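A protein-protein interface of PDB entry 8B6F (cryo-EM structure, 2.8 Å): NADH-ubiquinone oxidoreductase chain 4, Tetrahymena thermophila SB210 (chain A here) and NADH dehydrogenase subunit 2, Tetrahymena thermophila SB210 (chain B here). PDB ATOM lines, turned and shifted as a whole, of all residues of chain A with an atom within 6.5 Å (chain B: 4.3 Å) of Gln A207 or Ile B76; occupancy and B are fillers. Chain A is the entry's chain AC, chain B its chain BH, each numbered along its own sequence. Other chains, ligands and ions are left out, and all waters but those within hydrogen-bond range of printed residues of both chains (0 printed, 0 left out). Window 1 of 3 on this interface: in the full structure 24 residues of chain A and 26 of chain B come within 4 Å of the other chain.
Printed residues of chain B that touch a printed residue of chain A: Leu B71, Ile B76, Pro B77, Pro B78 and Met B112. Hydrophobic or aromatic side chains of chain A within 4 Å of the printed part of chain B: Leu A179 and Ile A180.
Printed residues of chain B within 4 Å of Leu A179: Ile B76. Of the printed residues of chain B, Ile A180 touches Leu B71 (3.6 Å), Ile B76 (3.4 Å) and Pro B78 (3.3 Å). Of the printed residues of chain A, Ile B76 touches Leu A179, Ile A180 and Gln A207. Printed residues of chain A within 4 Å of Pro B77: Glu A176 (3.4 Å) and Gln A207 (3.8 Å). The nearest residue of chain B that does not touch Gln A207 is Gly B75 (4.1 Å). The nearest residue of chain A that does not touch Ile B76 is Val A203 (4.4 Å). The nearest printed residue of chain B that does not touch Leu A179 is Pro B77 (4.7 Å).
OE1 of Gln A207 lies within hydrogen-bond range of OG of Ser A210 (3.4 Å). The side-chain hydroxyl (OG) of Ser A210 sits at hydrogen-bond distance from the side-chain carboxylate (OE1) of Glu A176. N of Ile B76 sits at hydrogen-bond distance from O of Leu B71 (3.2 Å).
Among the printed residues, merely in contact across the chains: Glu A176 with Pro B77, Leu A179 with Ile B76, Ile A180 with Leu B71, Ile A180 with Ile B76, Ile A180 with Pro B78, Gln A207 with Ile B76, Gln A207 with Pro B77 and Gln A207 with Met B112.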
ATOM      1  N   GLU A 176      23.683   1.280 -22.817  1.00  0.00           N
ATOM      2  CA  GLU A 176      23.946   0.064 -23.573  1.00  0.00           C
ATOM      3  C   GLU A 176      25.230   0.130 -24.389  1.00  0.00           C
ATOM      4  O   GLU A 176      25.724  -0.915 -24.823  1.00  0.00           O
ATOM      5  CB  GLU A 176      22.768  -0.228 -24.504  1.00  0.00           C
ATOM      6  CG  GLU A 176      21.472  -0.533 -23.780  1.00  0.00           C
ATOM      7  CD  GLU A 176      21.552  -1.798 -22.951  1.00  0.00           C
ATOM      8  OE1 GLU A 176      22.495  -2.590 -23.162  1.00  0.00           O
ATOM      9  OE2 GLU A 176      20.677  -1.998 -22.084  1.00  0.00           O
ATOM     10  N   LEU A 179      29.005  -1.840 -23.470  1.00  0.00           N
ATOM     11  CA  LEU A 179      29.349  -3.253 -23.579  1.00  0.00           C
ATOM     12  C   LEU A 179      30.531  -3.470 -24.518  1.00  0.00           C
ATOM     13  O   LEU A 179      31.482  -4.180 -24.174  1.00  0.00           O
ATOM     14  CB  LEU A 179      28.133  -4.055 -24.047  1.00  0.00           C
ATOM     15  CG  LEU A 179      28.302  -5.581 -24.101  1.00  0.00           C
ATOM     16  CD1 LEU A 179      26.957  -6.256 -23.956  1.00  0.00           C
ATOM     17  CD2 LEU A 179      28.965  -6.056 -25.387  1.00  0.00           C
ATOM     18  N   ILE A 180      30.493  -2.870 -25.711  1.00  0.00           N
ATOM     19  CA  ILE A 180      31.480  -3.211 -26.737  1.00  0.00           C
ATOM     20  C   ILE A 180      32.901  -2.910 -26.281  1.00  0.00           C
ATOM     21  O   ILE A 180      33.748  -3.815 -26.344  1.00  0.00           O
ATOM     22  CB  ILE A 180      31.131  -2.507 -28.062  1.00  0.00           C
ATOM     23  CG1 ILE A 180      29.906  -3.136 -28.735  1.00  0.00           C
ATOM     24  CG2 ILE A 180      32.321  -2.527 -29.023  1.00  0.00           C
ATOM     25  CD1 ILE A 180      30.094  -4.575 -29.156  1.00  0.00           C
ATOM     26  N   PHE A 202      30.542 -12.825 -19.472  1.00  0.00           N
ATOM     27  CA  PHE A 202      30.216 -11.427 -19.214  1.00  0.00           C
ATOM     28  C   PHE A 202      29.191 -10.913 -20.217  1.00  0.00           C
ATOM     29  O   PHE A 202      28.188 -10.299 -19.838  1.00  0.00           O
ATOM     30  CB  PHE A 202      31.495 -10.590 -19.270  1.00  0.00           C
ATOM     31  CG  PHE A 202      31.258  -9.116 -19.415  1.00  0.00           C
ATOM     32  CD1 PHE A 202      31.023  -8.330 -18.300  1.00  0.00           C
ATOM     33  CD2 PHE A 202      31.304  -8.509 -20.658  1.00  0.00           C
ATOM     34  CE1 PHE A 202      30.815  -6.972 -18.422  1.00  0.00           C
ATOM     35  CE2 PHE A 202      31.097  -7.150 -20.787  1.00  0.00           C
ATOM     36  CZ  PHE A 202      30.854  -6.379 -19.668  1.00  0.00           C
ATOM     37  N   VAL A 203      29.431 -11.153 -21.505  1.00  0.00           N
ATOM     38  CA  VAL A 203      28.544 -10.626 -22.540  1.00  0.00           C
ATOM     39  C   VAL A 203      27.131 -11.166 -22.359  1.00  0.00           C
ATOM     40  O   VAL A 203      26.154 -10.411 -22.361  1.00  0.00           O
ATOM     41  CB  VAL A 203      29.101 -10.955 -23.937  1.00  0.00           C
ATOM     42  CG1 VAL A 203      28.054 -10.709 -25.019  1.00  0.00           C
ATOM     43  CG2 VAL A 203      30.344 -10.134 -24.215  1.00  0.00           C
ATOM     44  N   ILE A 204      26.999 -12.484 -22.203  1.00  0.00           N
ATOM     45  CA  ILE A 204      25.669 -13.082 -22.149  1.00  0.00           C
ATOM     46  C   ILE A 204      24.932 -12.642 -20.888  1.00  0.00           C
ATOM     47  O   ILE A 204      23.753 -12.276 -20.938  1.00  0.00           O
ATOM     48  CB  ILE A 204      25.767 -14.617 -22.257  1.00  0.00           C
ATOM     49  CG1 ILE A 204      24.379 -15.238 -22.427  1.00  0.00           C
ATOM     50  CG2 ILE A 204      26.451 -15.225 -21.043  1.00  0.00           C
ATOM     51  CD1 ILE A 204      23.701 -14.878 -23.732  1.00  0.00           C
ATOM     52  N   TRP A 205      25.610 -12.671 -19.738  1.00  0.00           N
ATOM     53  CA  TRP A 205      24.942 -12.316 -18.489  1.00  0.00           C
ATOM     54  C   TRP A 205      24.506 -10.858 -18.486  1.00  0.00           C
ATOM     55  O   TRP A 205      23.396 -10.535 -18.051  1.00  0.00           O
ATOM     56  CB  TRP A 205      25.857 -12.598 -17.301  1.00  0.00           C
ATOM     57  CG  TRP A 205      25.445 -13.786 -16.492  1.00  0.00           C
ATOM     58  CD1 TRP A 205      24.509 -13.813 -15.502  1.00  0.00           C
ATOM     59  CD2 TRP A 205      25.957 -15.119 -16.597  1.00  0.00           C
ATOM     60  NE1 TRP A 205      24.406 -15.080 -14.983  1.00  0.00           N
ATOM     61  CE2 TRP A 205      25.284 -15.900 -15.639  1.00  0.00           C
ATOM     62  CE3 TRP A 205      26.920 -15.728 -17.407  1.00  0.00           C
ATOM     63  CZ2 TRP A 205      25.542 -17.257 -15.470  1.00  0.00           C
ATOM     64  CZ3 TRP A 205      27.173 -17.075 -17.239  1.00  0.00           C
ATOM     65  CH2 TRP A 205      26.486 -17.826 -16.276  1.00  0.00           C
ATOM     66  N   THR A 206      25.370  -9.958 -18.961  1.00  0.00           N
ATOM     67  CA  THR A 206      25.000  -8.549 -19.005  1.00  0.00           C
ATOM     68  C   THR A 206      23.939  -8.282 -20.060  1.00  0.00           C
ATOM     69  O   THR A 206      23.102  -7.391 -19.883  1.00  0.00           O
ATOM     70  CB  THR A 206      26.232  -7.683 -19.268  1.00  0.00           C
ATOM     71  OG1 THR A 206      26.847  -8.077 -20.500  1.00  0.00           O
ATOM     72  CG2 THR A 206      27.235  -7.820 -18.132  1.00  0.00           C
ATOM     73  N   GLN A 207      23.958  -9.031 -21.165  1.00  0.00           N
ATOM     74  CA  GLN A 207      22.993  -8.785 -22.230  1.00  0.00           C
ATOM     75  C   GLN A 207      21.598  -9.268 -21.861  1.00  0.00           C
ATOM     76  O   GLN A 207      20.609  -8.713 -22.350  1.00  0.00           O
ATOM     77  CB  GLN A 207      23.450  -9.451 -23.524  1.00  0.00           C
ATOM     78  CG  GLN A 207      24.473  -8.644 -24.300  1.00  0.00           C
ATOM     79  CD  GLN A 207      23.917  -7.311 -24.763  1.00  0.00           C
ATOM     80  OE1 GLN A 207      24.078  -6.291 -24.095  1.00  0.00           O
ATOM     81  NE2 GLN A 207      23.241  -7.318 -25.906  1.00  0.00           N
ATOM     82  N   LEU A 208      21.489 -10.288 -21.012  1.00  0.00           N
ATOM     83  CA  LEU A 208      20.171 -10.686 -20.533  1.00  0.00           C
ATOM     84  C   LEU A 208      19.510  -9.540 -19.780  1.00  0.00           C
ATOM     85  O   LEU A 208      18.341  -9.217 -20.013  1.00  0.00           O
ATOM     86  CB  LEU A 208      20.276 -11.934 -19.657  1.00  0.00           C
ATOM     87  CG  LEU A 208      18.950 -12.525 -19.168  1.00  0.00           C
ATOM     88  CD1 LEU A 208      17.980 -12.761 -20.315  1.00  0.00           C
ATOM     89  CD2 LEU A 208      19.196 -13.821 -18.421  1.00  0.00           C
ATOM     90  N   GLY A 209      20.252  -8.910 -18.869  1.00  0.00           N
ATOM     91  CA  GLY A 209      19.715  -7.758 -18.164  1.00  0.00           C
ATOM     92  C   GLY A 209      19.485  -6.571 -19.080  1.00  0.00           C
ATOM     93  O   GLY A 209      18.527  -5.817 -18.904  1.00  0.00           O
ATOM     94  N   SER A 210      20.355  -6.395 -20.077  1.00  0.00           N
ATOM     95  CA  SER A 210      20.152  -5.338 -21.060  1.00  0.00           C
ATOM     96  C   SER A 210      18.845  -5.539 -21.812  1.00  0.00           C
ATOM     97  O   SER A 210      18.121  -4.574 -22.084  1.00  0.00           O
ATOM     98  CB  SER A 210      21.327  -5.291 -22.035  1.00  0.00           C
ATOM     99  OG  SER A 210      22.535  -4.976 -21.363  1.00  0.00           O
ATOM    100  N   LEU A 211      18.530  -6.785 -22.162  1.00  0.00           N
ATOM    101  CA  LEU A 211      17.255  -7.065 -22.812  1.00  0.00           C
ATOM    102  C   LEU A 211      16.085  -6.776 -21.880  1.00  0.00           C
ATOM    103  O   LEU A 211      15.059  -6.247 -22.318  1.00  0.00           O
ATOM    104  CB  LEU A 211      17.218  -8.519 -23.282  1.00  0.00           C
ATOM    105  CG  LEU A 211      18.145  -8.889 -24.445  1.00  0.00           C
ATOM    106  CD1 LEU A 211      18.040 -10.374 -24.747  1.00  0.00           C
ATOM    107  CD2 LEU A 211      17.838  -8.070 -25.692  1.00  0.00           C
ATOM    108  N   LEU A 212      16.217  -7.105 -20.594  1.00  0.00           N
ATOM    109  CA  LEU A 212      15.155  -6.782 -19.645  1.00  0.00           C
ATOM    110  C   LEU A 212      14.915  -5.279 -19.581  1.00  0.00           C
ATOM    111  O   LEU A 212      13.770  -4.819 -19.625  1.00  0.00           O
ATOM    112  CB  LEU A 212      15.506  -7.331 -18.262  1.00  0.00           C
ATOM    113  CG  LEU A 212      15.523  -8.855 -18.108  1.00  0.00           C
ATOM    114  CD1 LEU A 212      15.967  -9.251 -16.713  1.00  0.00           C
ATOM    115  CD2 LEU A 212      14.166  -9.449 -18.413  1.00  0.00           C
ATOM    116  N   PHE A 255      21.340  -7.495 -13.081  1.00  0.00           N
ATOM    117  CA  PHE A 255      22.259  -8.310 -13.865  1.00  0.00           C
ATOM    118  C   PHE A 255      23.608  -7.617 -14.005  1.00  0.00           C
ATOM    119  O   PHE A 255      24.659  -8.255 -13.882  1.00  0.00           O
ATOM    120  CB  PHE A 255      21.659  -8.599 -15.238  1.00  0.00           C
ATOM    121  CG  PHE A 255      20.843  -9.858 -15.291  1.00  0.00           C
ATOM    122  CD1 PHE A 255      21.458 -11.096 -15.315  1.00  0.00           C
ATOM    123  CD2 PHE A 255      19.460  -9.799 -15.329  1.00  0.00           C
ATOM    124  CE1 PHE A 255      20.708 -12.253 -15.369  1.00  0.00           C
ATOM    125  CE2 PHE A 255      18.704 -10.952 -15.384  1.00  0.00           C
ATOM    126  CZ  PHE A 255      19.329 -12.181 -15.404  1.00  0.00           C
ATOM    127  N   LEU B  71      28.911  -9.806 -33.798  1.00  0.00           N
ATOM    128  CA  LEU B  71      28.218  -9.070 -32.749  1.00  0.00           C
ATOM    129  C   LEU B  71      26.936  -8.446 -33.280  1.00  0.00           C
ATOM    130  O   LEU B  71      25.900  -8.468 -32.607  1.00  0.00           O
ATOM    131  CB  LEU B  71      29.140  -8.002 -32.161  1.00  0.00           C
ATOM    132  CG  LEU B  71      30.389  -8.513 -31.432  1.00  0.00           C
ATOM    133  CD1 LEU B  71      31.280  -7.352 -31.038  1.00  0.00           C
ATOM    134  CD2 LEU B  71      30.032  -9.340 -30.210  1.00  0.00           C
ATOM    135  N   ALA B  74      24.361 -11.037 -33.557  1.00  0.00           N
ATOM    136  CA  ALA B  74      23.877 -11.369 -32.223  1.00  0.00           C
ATOM    137  C   ALA B  74      22.861 -10.347 -31.734  1.00  0.00           C
ATOM    138  O   ALA B  74      21.847 -10.710 -31.126  1.00  0.00           O
ATOM    139  CB  ALA B  74      25.054 -11.462 -31.253  1.00  0.00           C
ATOM    140  N   GLY B  75      23.116  -9.065 -31.982  1.00  0.00           N
ATOM    141  CA  GLY B  75      22.203  -8.013 -31.581  1.00  0.00           C
ATOM    142  C   GLY B  75      22.774  -7.109 -30.510  1.00  0.00           C
ATOM    143  O   GLY B  75      22.030  -6.550 -29.700  1.00  0.00           O
ATOM    144  N   ILE B  76      24.091  -6.956 -30.495  1.00  0.00           N
ATOM    145  CA  ILE B  76      24.735  -6.100 -29.492  1.00  0.00           C
ATOM    146  C   ILE B  76      24.321  -4.653 -29.739  1.00  0.00           C
ATOM    147  O   ILE B  76      24.172  -4.253 -30.907  1.00  0.00           O
ATOM    148  CB  ILE B  76      26.255  -6.279 -29.547  1.00  0.00           C
ATOM    149  CG1 ILE B  76      26.631  -7.764 -29.525  1.00  0.00           C
ATOM    150  CG2 ILE B  76      26.932  -5.605 -28.381  1.00  0.00           C
ATOM    151  CD1 ILE B  76      26.065  -8.546 -28.358  1.00  0.00           C
ATOM    152  N   PRO B  77      24.118  -3.839 -28.703  1.00  0.00           N
ATOM    153  CA  PRO B  77      23.330  -2.604 -28.862  1.00  0.00           C
ATOM    154  C   PRO B  77      23.841  -1.701 -29.973  1.00  0.00           C
ATOM    155  O   PRO B  77      23.080  -1.364 -30.892  1.00  0.00           O
ATOM    156  CB  PRO B  77      23.450  -1.930 -27.488  1.00  0.00           C
ATOM    157  CG  PRO B  77      23.656  -3.060 -26.554  1.00  0.00           C
ATOM    158  CD  PRO B  77      24.500  -4.046 -27.292  1.00  0.00           C
ATOM    159  N   PRO B  78      25.105  -1.276 -29.944  1.00  0.00           N
ATOM    160  CA  PRO B  78      25.526  -0.227 -30.891  1.00  0.00           C
ATOM    161  C   PRO B  78      25.389  -0.618 -32.351  1.00  0.00           C
ATOM    162  O   PRO B  78      25.325   0.272 -33.207  1.00  0.00           O
ATOM    163  CB  PRO B  78      26.994   0.017 -30.519  1.00  0.00           C
ATOM    164  CG  PRO B  78      27.434  -1.229 -29.866  1.00  0.00           C
ATOM    165  CD  PRO B  78      26.239  -1.775 -29.147  1.00  0.00           C
ATOM    166  N   LEU B  79      25.334  -1.907 -32.665  1.00  0.00           N
ATOM    167  CA  LEU B  79      25.432  -2.373 -34.038  1.00  0.00           C
ATOM    168  C   LEU B  79      24.062  -2.397 -34.714  1.00  0.00           C
ATOM    169  O   LEU B  79      23.040  -2.030 -34.132  1.00  0.00           O
ATOM    170  CB  LEU B  79      26.098  -3.747 -34.064  1.00  0.00           C
ATOM    171  CG  LEU B  79      27.470  -3.779 -33.382  1.00  0.00           C
ATOM    172  CD1 LEU B  79      28.056  -5.173 -33.410  1.00  0.00           C
ATOM    173  CD2 LEU B  79      28.431  -2.793 -34.025  1.00  0.00           C
ATOM    174  N   PHE B  82      20.818  -4.629 -33.678  1.00  0.00           N
ATOM    175  CA  PHE B  82      20.109  -4.145 -32.501  1.00  0.00           C
ATOM    176  C   PHE B  82      18.945  -3.242 -32.881  1.00  0.00           C
ATOM    177  O   PHE B  82      17.879  -3.298 -32.258  1.00  0.00           O
ATOM    178  CB  PHE B  82      21.063  -3.394 -31.579  1.00  0.00           C
ATOM    179  CG  PHE B  82      20.364  -2.524 -30.575  1.00  0.00           C
ATOM    180  CD1 PHE B  82      19.825  -3.070 -29.422  1.00  0.00           C
ATOM    181  CD2 PHE B  82      20.242  -1.160 -30.787  1.00  0.00           C
ATOM    182  CE1 PHE B  82      19.184  -2.272 -28.499  1.00  0.00           C
ATOM    183  CE2 PHE B  82      19.601  -0.357 -29.868  1.00  0.00           C
ATOM    184  CZ  PHE B  82      19.072  -0.913 -28.722  1.00  0.00           C
ATOM    185  N   MET B 112      21.637 -15.054 -29.440  1.00  0.00           N
ATOM    186  CA  MET B 112      22.787 -14.221 -29.108  1.00  0.00           C
ATOM    187  C   MET B 112      23.966 -15.073 -28.663  1.00  0.00           C
ATOM    188  O   MET B 112      25.095 -14.877 -29.124  1.00  0.00           O
ATOM    189  CB  MET B 112      22.401 -13.214 -28.027  1.00  0.00           C
ATOM    190  CG  MET B 112      23.545 -12.320 -27.575  1.00  0.00           C
ATOM    191  SD  MET B 112      23.048 -11.131 -26.319  1.00  0.00           S
ATOM    192  CE  MET B 112      21.853 -10.144 -27.224  1.00  0.00           C
